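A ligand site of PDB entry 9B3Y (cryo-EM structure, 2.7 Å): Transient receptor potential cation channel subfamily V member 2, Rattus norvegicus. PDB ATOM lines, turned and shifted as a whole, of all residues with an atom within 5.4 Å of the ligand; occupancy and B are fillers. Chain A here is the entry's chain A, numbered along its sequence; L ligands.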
ATOM      1  N   PHE A 395       0.007   1.625  20.121  1.00  0.00           N
ATOM      2  CA  PHE A 395       1.158   2.380  20.610  1.00  0.00           C
ATOM      3  C   PHE A 395       1.669   1.807  21.945  1.00  0.00           C
ATOM      4  O   PHE A 395       2.864   1.537  22.077  1.00  0.00           O
ATOM      5  CB  PHE A 395       0.762   3.856  20.740  1.00  0.00           C
ATOM      6  CG  PHE A 395       1.836   4.728  21.338  1.00  0.00           C
ATOM      7  CD1 PHE A 395       2.987   5.048  20.589  1.00  0.00           C
ATOM      8  CD2 PHE A 395       1.693   5.236  22.639  1.00  0.00           C
ATOM      9  CE1 PHE A 395       3.983   5.864  21.144  1.00  0.00           C
ATOM     10  CE2 PHE A 395       2.681   6.060  23.185  1.00  0.00           C
ATOM     11  CZ  PHE A 395       3.820   6.376  22.444  1.00  0.00           C
ATOM     12  N   ASN A 396       0.782   1.545  22.901  1.00  0.00           N
ATOM     13  CA  ASN A 396       1.133   0.922  24.181  1.00  0.00           C
ATOM     14  C   ASN A 396       1.773  -0.460  24.016  1.00  0.00           C
ATOM     15  O   ASN A 396       2.744  -0.783  24.707  1.00  0.00           O
ATOM     16  CB  ASN A 396      -0.133   0.837  25.043  1.00  0.00           C
ATOM     17  CG  ASN A 396      -0.659   2.174  25.561  1.00  0.00           C
ATOM     18  OD1 ASN A 396      -0.141   3.247  25.320  1.00  0.00           O
ATOM     19  ND2 ASN A 396      -1.689   2.137  26.365  1.00  0.00           N
ATOM     20  N   PHE A 397       1.301  -1.265  23.069  1.00  0.00           N
ATOM     21  CA  PHE A 397       1.898  -2.524  22.634  1.00  0.00           C
ATOM     22  C   PHE A 397       3.287  -2.363  22.016  1.00  0.00           C
ATOM     23  O   PHE A 397       4.187  -3.113  22.366  1.00  0.00           O
ATOM     24  CB  PHE A 397       0.954  -3.195  21.631  1.00  0.00           C
ATOM     25  CG  PHE A 397       1.512  -4.419  20.926  1.00  0.00           C
ATOM     26  CD1 PHE A 397       1.946  -5.534  21.659  1.00  0.00           C
ATOM     27  CD2 PHE A 397       1.576  -4.446  19.523  1.00  0.00           C
ATOM     28  CE1 PHE A 397       2.392  -6.687  20.997  1.00  0.00           C
ATOM     29  CE2 PHE A 397       2.054  -5.591  18.861  1.00  0.00           C
ATOM     30  CZ  PHE A 397       2.446  -6.713  19.594  1.00  0.00           C
ATOM     31  N   ALA A 398       3.486  -1.393  21.122  1.00  0.00           N
ATOM     32  CA  ALA A 398       4.785  -1.121  20.492  1.00  0.00           C
ATOM     33  C   ALA A 398       5.837  -0.631  21.496  1.00  0.00           C
ATOM     34  O   ALA A 398       6.968  -1.082  21.445  1.00  0.00           O
ATOM     35  CB  ALA A 398       4.565  -0.125  19.361  1.00  0.00           C
ATOM     36  N   CYS A 399       5.481   0.221  22.469  1.00  0.00           N
ATOM     37  CA  CYS A 399       6.378   0.567  23.575  1.00  0.00           C
ATOM     38  C   CYS A 399       6.787  -0.664  24.382  1.00  0.00           C
ATOM     39  O   CYS A 399       7.953  -0.802  24.744  1.00  0.00           O
ATOM     40  CB  CYS A 399       5.687   1.570  24.495  1.00  0.00           C
ATOM     41  SG  CYS A 399       5.529   3.168  23.692  1.00  0.00           S
ATOM     42  N   TYR A 400       5.843  -1.557  24.648  1.00  0.00           N
ATOM     43  CA  TYR A 400       6.115  -2.768  25.405  1.00  0.00           C
ATOM     44  C   TYR A 400       6.932  -3.781  24.590  1.00  0.00           C
ATOM     45  O   TYR A 400       7.823  -4.407  25.144  1.00  0.00           O
ATOM     46  CB  TYR A 400       4.801  -3.329  25.919  1.00  0.00           C
ATOM     47  CG  TYR A 400       4.999  -4.425  26.936  1.00  0.00           C
ATOM     48  CD1 TYR A 400       5.299  -4.100  28.263  1.00  0.00           C
ATOM     49  CD2 TYR A 400       4.948  -5.760  26.521  1.00  0.00           C
ATOM     50  CE1 TYR A 400       5.555  -5.132  29.186  1.00  0.00           C
ATOM     51  CE2 TYR A 400       5.184  -6.788  27.443  1.00  0.00           C
ATOM     52  CZ  TYR A 400       5.504  -6.468  28.772  1.00  0.00           C
ATOM     53  OH  TYR A 400       5.804  -7.445  29.631  1.00  0.00           O
ATOM     54  N   VAL A 402       9.265  -2.767  22.332  1.00  0.00           N
ATOM     55  CA  VAL A 402      10.584  -2.112  22.390  1.00  0.00           C
ATOM     56  C   VAL A 402      11.243  -2.318  23.748  1.00  0.00           C
ATOM     57  O   VAL A 402      12.425  -2.624  23.814  1.00  0.00           O
ATOM     58  CB  VAL A 402      10.473  -0.622  22.033  1.00  0.00           C
ATOM     59  CG1 VAL A 402      11.761   0.150  22.310  1.00  0.00           C
ATOM     60  CG2 VAL A 402      10.148  -0.469  20.550  1.00  0.00           C
ATOM     61  N   TYR A 403      10.492  -2.187  24.843  1.00  0.00           N
ATOM     62  CA  TYR A 403      10.963  -2.533  26.187  1.00  0.00           C
ATOM     63  C   TYR A 403      11.357  -4.006  26.285  1.00  0.00           C
ATOM     64  O   TYR A 403      12.447  -4.303  26.754  1.00  0.00           O
ATOM     65  CB  TYR A 403       9.876  -2.152  27.200  1.00  0.00           C
ATOM     66  CG  TYR A 403      10.007  -2.714  28.609  1.00  0.00           C
ATOM     67  CD1 TYR A 403      10.957  -2.205  29.507  1.00  0.00           C
ATOM     68  CD2 TYR A 403       9.125  -3.721  29.030  1.00  0.00           C
ATOM     69  CE1 TYR A 403      11.016  -2.692  30.830  1.00  0.00           C
ATOM     70  CE2 TYR A 403       9.182  -4.216  30.347  1.00  0.00           C
ATOM     71  CZ  TYR A 403      10.115  -3.689  31.242  1.00  0.00           C
ATOM     72  OH  TYR A 403      10.143  -4.132  32.530  1.00  0.00           O
ATOM     73  N   GLY A 444      11.908   1.617  32.566  1.00  0.00           N
ATOM     74  CA  GLY A 444      10.726   0.875  32.131  1.00  0.00           C
ATOM     75  C   GLY A 444      10.098   0.026  33.245  1.00  0.00           C
ATOM     76  O   GLY A 444       8.885  -0.052  33.356  1.00  0.00           O
ATOM     77  N   TYR A 447       8.502   2.658  35.665  1.00  0.00           N
ATOM     78  CA  TYR A 447       7.298   3.150  34.979  1.00  0.00           C
ATOM     79  C   TYR A 447       6.141   2.159  35.081  1.00  0.00           C
ATOM     80  O   TYR A 447       5.045   2.530  35.495  1.00  0.00           O
ATOM     81  CB  TYR A 447       7.621   3.458  33.521  1.00  0.00           C
ATOM     82  CG  TYR A 447       6.425   3.975  32.766  1.00  0.00           C
ATOM     83  CD1 TYR A 447       5.487   3.084  32.218  1.00  0.00           C
ATOM     84  CD2 TYR A 447       6.197   5.360  32.686  1.00  0.00           C
ATOM     85  CE1 TYR A 447       4.292   3.555  31.656  1.00  0.00           C
ATOM     86  CE2 TYR A 447       5.017   5.848  32.101  1.00  0.00           C
ATOM     87  CZ  TYR A 447       4.043   4.950  31.616  1.00  0.00           C
ATOM     88  OH  TYR A 447       2.873   5.413  31.128  1.00  0.00           O
ATOM     89  N   LEU A 448       6.372   0.884  34.753  1.00  0.00           N
ATOM     90  CA  LEU A 448       5.356  -0.160  34.882  1.00  0.00           C
ATOM     91  C   LEU A 448       4.998  -0.439  36.341  1.00  0.00           C
ATOM     92  O   LEU A 448       3.819  -0.666  36.625  1.00  0.00           O
ATOM     93  CB  LEU A 448       5.850  -1.450  34.191  1.00  0.00           C
ATOM     94  CG  LEU A 448       5.913  -1.356  32.664  1.00  0.00           C
ATOM     95  CD1 LEU A 448       6.667  -2.566  32.119  1.00  0.00           C
ATOM     96  CD2 LEU A 448       4.532  -1.360  32.030  1.00  0.00           C
ATOM     97  N   GLN A 452       1.057   0.139  37.476  1.00  0.00           N
ATOM     98  CA  GLN A 452       0.247  -0.910  38.106  1.00  0.00           C
ATOM     99  C   GLN A 452      -0.119  -0.620  39.568  1.00  0.00           C
ATOM    100  O   GLN A 452      -1.214  -0.959  39.999  1.00  0.00           O
ATOM    101  CB  GLN A 452       0.938  -2.272  38.003  1.00  0.00           C
ATOM    102  CG  GLN A 452       1.099  -2.780  36.567  1.00  0.00           C
ATOM    103  CD  GLN A 452      -0.211  -2.833  35.784  1.00  0.00           C
ATOM    104  OE1 GLN A 452      -0.368  -2.175  34.769  1.00  0.00           O
ATOM    105  NE2 GLN A 452      -1.191  -3.596  36.203  1.00  0.00           N
ATOM    106  N   GLU A 473      -3.169  -7.840  35.147  1.00  0.00           N
ATOM    107  CA  GLU A 473      -2.856  -6.665  35.971  1.00  0.00           C
ATOM    108  C   GLU A 473      -1.958  -7.006  37.163  1.00  0.00           C
ATOM    109  O   GLU A 473      -1.186  -6.163  37.607  1.00  0.00           O
ATOM    110  CB  GLU A 473      -4.165  -5.962  36.387  1.00  0.00           C
ATOM    111  CG  GLU A 473      -5.035  -5.525  35.197  1.00  0.00           C
ATOM    112  CD  GLU A 473      -4.286  -4.722  34.122  1.00  0.00           C
ATOM    113  OE1 GLU A 473      -3.382  -3.921  34.447  1.00  0.00           O
ATOM    114  OE2 GLU A 473      -4.551  -4.928  32.915  1.00  0.00           O
ATOM    115  N   PHE A 476       1.750  -7.987  35.222  1.00  0.00           N
ATOM    116  CA  PHE A 476       2.500  -6.767  34.945  1.00  0.00           C
ATOM    117  C   PHE A 476       3.093  -6.143  36.223  1.00  0.00           C
ATOM    118  O   PHE A 476       4.135  -5.491  36.138  1.00  0.00           O
ATOM    119  CB  PHE A 476       1.606  -5.779  34.181  1.00  0.00           C
ATOM    120  CG  PHE A 476       1.603  -5.931  32.673  1.00  0.00           C
ATOM    121  CD1 PHE A 476       0.791  -6.882  32.030  1.00  0.00           C
ATOM    122  CD2 PHE A 476       2.379  -5.066  31.877  1.00  0.00           C
ATOM    123  CE1 PHE A 476       0.744  -6.960  30.632  1.00  0.00           C
ATOM    124  CE2 PHE A 476       2.322  -5.142  30.478  1.00  0.00           C
ATOM    125  CZ  PHE A 476       1.501  -6.081  29.854  1.00  0.00           C
ATOM    126  N   TYR A 514      -1.086 -10.389  26.573  1.00  0.00           N
ATOM    127  CA  TYR A 514      -2.189  -9.483  26.901  1.00  0.00           C
ATOM    128  C   TYR A 514      -2.764  -8.851  25.634  1.00  0.00           C
ATOM    129  O   TYR A 514      -3.971  -8.890  25.410  1.00  0.00           O
ATOM    130  CB  TYR A 514      -1.708  -8.399  27.880  1.00  0.00           C
ATOM    131  CG  TYR A 514      -2.690  -7.261  28.063  1.00  0.00           C
ATOM    132  CD1 TYR A 514      -3.793  -7.401  28.916  1.00  0.00           C
ATOM    133  CD2 TYR A 514      -2.511  -6.072  27.352  1.00  0.00           C
ATOM    134  CE1 TYR A 514      -4.728  -6.360  29.037  1.00  0.00           C
ATOM    135  CE2 TYR A 514      -3.453  -5.026  27.450  1.00  0.00           C
ATOM    136  CZ  TYR A 514      -4.567  -5.174  28.282  1.00  0.00           C
ATOM    137  OH  TYR A 514      -5.489  -4.182  28.381  1.00  0.00           O
ATOM    138  N   TYR A 515      -1.899  -8.348  24.764  1.00  0.00           N
ATOM    139  CA  TYR A 515      -2.285  -7.551  23.593  1.00  0.00           C
ATOM    140  C   TYR A 515      -2.922  -8.363  22.470  1.00  0.00           C
ATOM    141  O   TYR A 515      -3.412  -7.786  21.506  1.00  0.00           O
ATOM    142  CB  TYR A 515      -1.073  -6.761  23.113  1.00  0.00           C
ATOM    143  CG  TYR A 515      -0.495  -5.844  24.176  1.00  0.00           C
ATOM    144  CD1 TYR A 515      -1.072  -4.596  24.406  1.00  0.00           C
ATOM    145  CD2 TYR A 515       0.618  -6.259  24.928  1.00  0.00           C
ATOM    146  CE1 TYR A 515      -0.542  -3.739  25.391  1.00  0.00           C
ATOM    147  CE2 TYR A 515       1.157  -5.412  25.907  1.00  0.00           C
ATOM    148  CZ  TYR A 515       0.573  -4.148  26.134  1.00  0.00           C
ATOM    149  OH  TYR A 515       1.108  -3.334  27.075  1.00  0.00           O
ATOM    150  N   TYR A 675      -2.646   8.067  31.312  1.00  0.00           N
ATOM    151  CA  TYR A 675      -1.563   7.432  32.059  1.00  0.00           C
ATOM    152  C   TYR A 675      -1.416   8.048  33.446  1.00  0.00           C
ATOM    153  O   TYR A 675      -1.817   9.195  33.660  1.00  0.00           O
ATOM    154  CB  TYR A 675      -0.250   7.569  31.270  1.00  0.00           C
ATOM    155  CG  TYR A 675      -0.255   7.100  29.830  1.00  0.00           C
ATOM    156  CD1 TYR A 675      -0.388   5.737  29.518  1.00  0.00           C
ATOM    157  CD2 TYR A 675      -0.064   8.038  28.798  1.00  0.00           C
ATOM    158  CE1 TYR A 675      -0.330   5.306  28.181  1.00  0.00           C
ATOM    159  CE2 TYR A 675      -0.006   7.607  27.462  1.00  0.00           C
ATOM    160  CZ  TYR A 675      -0.139   6.243  27.149  1.00  0.00           C
ATOM    161  OH  TYR A 675      -0.075   5.860  25.849  1.00  0.00           O
ATOM    162  N   TRP A 676      -0.793   7.355  34.388  1.00  0.00           N
ATOM    163  CA  TRP A 676      -0.624   7.815  35.777  1.00  0.00           C
ATOM    164  C   TRP A 676       0.025   9.212  35.900  1.00  0.00           C
ATOM    165  O   TRP A 676      -0.299   9.950  36.834  1.00  0.00           O
ATOM    166  CB  TRP A 676       0.186   6.755  36.535  1.00  0.00           C
ATOM    167  CG  TRP A 676       1.612   6.562  36.091  1.00  0.00           C
ATOM    168  CD1 TRP A 676       2.036   5.655  35.178  1.00  0.00           C
ATOM    169  CD2 TRP A 676       2.803   7.292  36.506  1.00  0.00           C
ATOM    170  NE1 TRP A 676       3.395   5.789  34.999  1.00  0.00           N
ATOM    171  CE2 TRP A 676       3.913   6.794  35.776  1.00  0.00           C
ATOM    172  CE3 TRP A 676       3.045   8.333  37.420  1.00  0.00           C
ATOM    173  CZ2 TRP A 676       5.205   7.321  35.923  1.00  0.00           C
ATOM    174  CZ3 TRP A 676       4.337   8.870  37.587  1.00  0.00           C
ATOM    175  CH2 TRP A 676       5.409   8.375  36.827  1.00  0.00           C
ATOM    176  N   TRP A 677       0.880   9.573  34.936  1.00  0.00           N
ATOM    177  CA  TRP A 677       1.593  10.858  34.813  1.00  0.00           C
ATOM    178  C   TRP A 677       0.891  11.909  33.931  1.00  0.00           C
ATOM    179  O   TRP A 677       1.288  13.070  33.945  1.00  0.00           O
ATOM    180  CB  TRP A 677       2.973  10.539  34.229  1.00  0.00           C
ATOM    181  CG  TRP A 677       2.978   9.924  32.860  1.00  0.00           C
ATOM    182  CD1 TRP A 677       2.839   8.599  32.599  1.00  0.00           C
ATOM    183  CD2 TRP A 677       3.099  10.561  31.556  1.00  0.00           C
ATOM    184  NE1 TRP A 677       2.848   8.392  31.243  1.00  0.00           N
ATOM    185  CE2 TRP A 677       2.972   9.565  30.546  1.00  0.00           C
ATOM    186  CE3 TRP A 677       3.309  11.892  31.118  1.00  0.00           C
ATOM    187  CZ2 TRP A 677       3.004   9.869  29.180  1.00  0.00           C
ATOM    188  CZ3 TRP A 677       3.352  12.200  29.744  1.00  0.00           C
ATOM    189  CH2 TRP A 677       3.182  11.203  28.777  1.00  0.00           C
HETATM  190  O1  LIG L   1      -1.594  -0.086  28.015  1.00  0.00           O
HETATM  191  O2  LIG L   1      -0.726   0.587  30.173  1.00  0.00           O
HETATM  192  P1  LIG L   1      -0.638  -0.425  29.093  1.00  0.00           P
HETATM  193  O3  LIG L   1       0.840  -0.546  28.498  1.00  0.00           O
HETATM  194  C1  LIG L   1       1.977  -0.113  29.262  1.00  0.00           C
HETATM  195  C2  LIG L   1       3.157   0.076  28.297  1.00  0.00           C
HETATM  196  C3  LIG L   1       2.897   1.232  27.313  1.00  0.00           C
HETATM  197  O4  LIG L   1       3.073   2.497  27.977  1.00  0.00           O
HETATM  198  C4  LIG L   1       3.221   3.613  27.218  1.00  0.00           C
HETATM  199  O5  LIG L   1       3.308   3.601  26.007  1.00  0.00           O
HETATM  200  C5  LIG L   1       3.673   4.780  28.077  1.00  0.00           C
HETATM  201  C6  LIG L   1       4.638   5.760  27.376  1.00  0.00           C
HETATM  202  C7  LIG L   1       5.406   6.602  28.421  1.00  0.00           C
HETATM  203  C8  LIG L   1       6.331   7.656  27.780  1.00  0.00           C
HETATM  204  C9  LIG L   1       7.320   8.304  28.787  1.00  0.00           C
HETATM  205  C10 LIG L   1       6.649   9.055  29.951  1.00  0.00           C
HETATM  206  C11 LIG L   1       7.679   9.821  30.814  1.00  0.00           C
HETATM  207  C12 LIG L   1       7.057  10.527  32.044  1.00  0.00           C
HETATM  208  C13 LIG L   1       6.740   9.551  33.199  1.00  0.00           C
HETATM  209  O6  LIG L   1       4.350   0.375  29.061  1.00  0.00           O
HETATM  210  C14 LIG L   1       5.554   0.251  28.436  1.00  0.00           C
HETATM  211  O7  LIG L   1       5.704  -0.217  27.329  1.00  0.00           O
HETATM  212  C15 LIG L   1       6.720   0.753  29.270  1.00  0.00           C
HETATM  213  C16 LIG L   1       7.052   2.229  28.950  1.00  0.00           C
HETATM  214  C17 LIG L   1       8.563   2.492  28.857  1.00  0.00           C
HETATM  215  C18 LIG L   1       9.171   2.061  27.501  1.00  0.00           C
HETATM  216  C19 LIG L   1       8.962   3.114  26.376  1.00  0.00           C
HETATM  217  C20 LIG L   1       9.545   2.659  25.023  1.00  0.00           C
HETATM  218  C21 LIG L   1       9.282   3.704  23.919  1.00  0.00           C
HETATM  219  C22 LIG L   1       9.589   3.170  22.505  1.00  0.00           C
HETATM  220  C23 LIG L   1       9.073   4.111  21.401  1.00  0.00           C
HETATM  221  O8  LIG L   1      -0.915  -1.928  29.605  1.00  0.00           O
HETATM  222  C24 LIG L   1      -0.365  -2.436  30.832  1.00  0.00           C
HETATM  223  C25 LIG L   1      -1.173  -3.711  31.208  1.00  0.00           C
HETATM  224  N1  LIG L   1      -2.545  -3.454  31.823  1.00  0.00           N
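ND2 of Asn 396 sits at hydrogen-bond distance from O1 of the ligand (2.8 Å). N of Tyr 400 is in hydrogen-bond range of O7 of the ligand (3.0 Å). The side-chain hydroxyl of Tyr 515 lies within hydrogen-bond range of an oxygen (O3) of the ligand, 3.1 Å away. N1 of the ligand is in salt-bridge range of OE2 of Glu 473 (2.7 Å). The side-chain sulfur of Cys 399 lies within hydrogen-bond range of an oxygen (O5) of the ligand, at 3.2 Å.
The side-chain amide oxygen (OD1) of Asn 396 sits at hydrogen-bond distance from the side-chain hydroxyl (OH) of Tyr 675, 2.7 Å away. The indole nitrogen (NE1) of Trp 677 lies within hydrogen-bond range of the side-chain hydroxyl (OH) of Tyr 447, at 3.0 Å. O of Phe 395 sits at hydrogen-bond distance from SG of Cys 399, 3.5 Å away. The side-chain carboxylate of Glu 473 sits at hydrogen-bond distance from the side-chain amide nitrogen of Gln 452, at 2.8 Å.
Merely in contact with the ligand: Phe 395, Val 402, Tyr 447, Leu 448, Gln 452, Phe 476, Trp 676 and Trp 677. Hydrophobic or aromatic side chains within 4 Å of the ligand: Phe 395, Tyr 400, Val 402, Tyr 447, Leu 448, Phe 476, Trp 676 and Trp 677. Within 4 Å of the ligand: Phe 395, Asn 396, Cys 399, Tyr 400, Val 402, Tyr 447, Leu 448, Gln 452, Glu 473, Phe 476, Tyr 515, Trp 676 and Trp 677. Along chain A the residues within 4 Å of the ligand span positions 395 to 677. The nearest printed residue that does not touch the ligand is Tyr 675 (4.04 Å).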
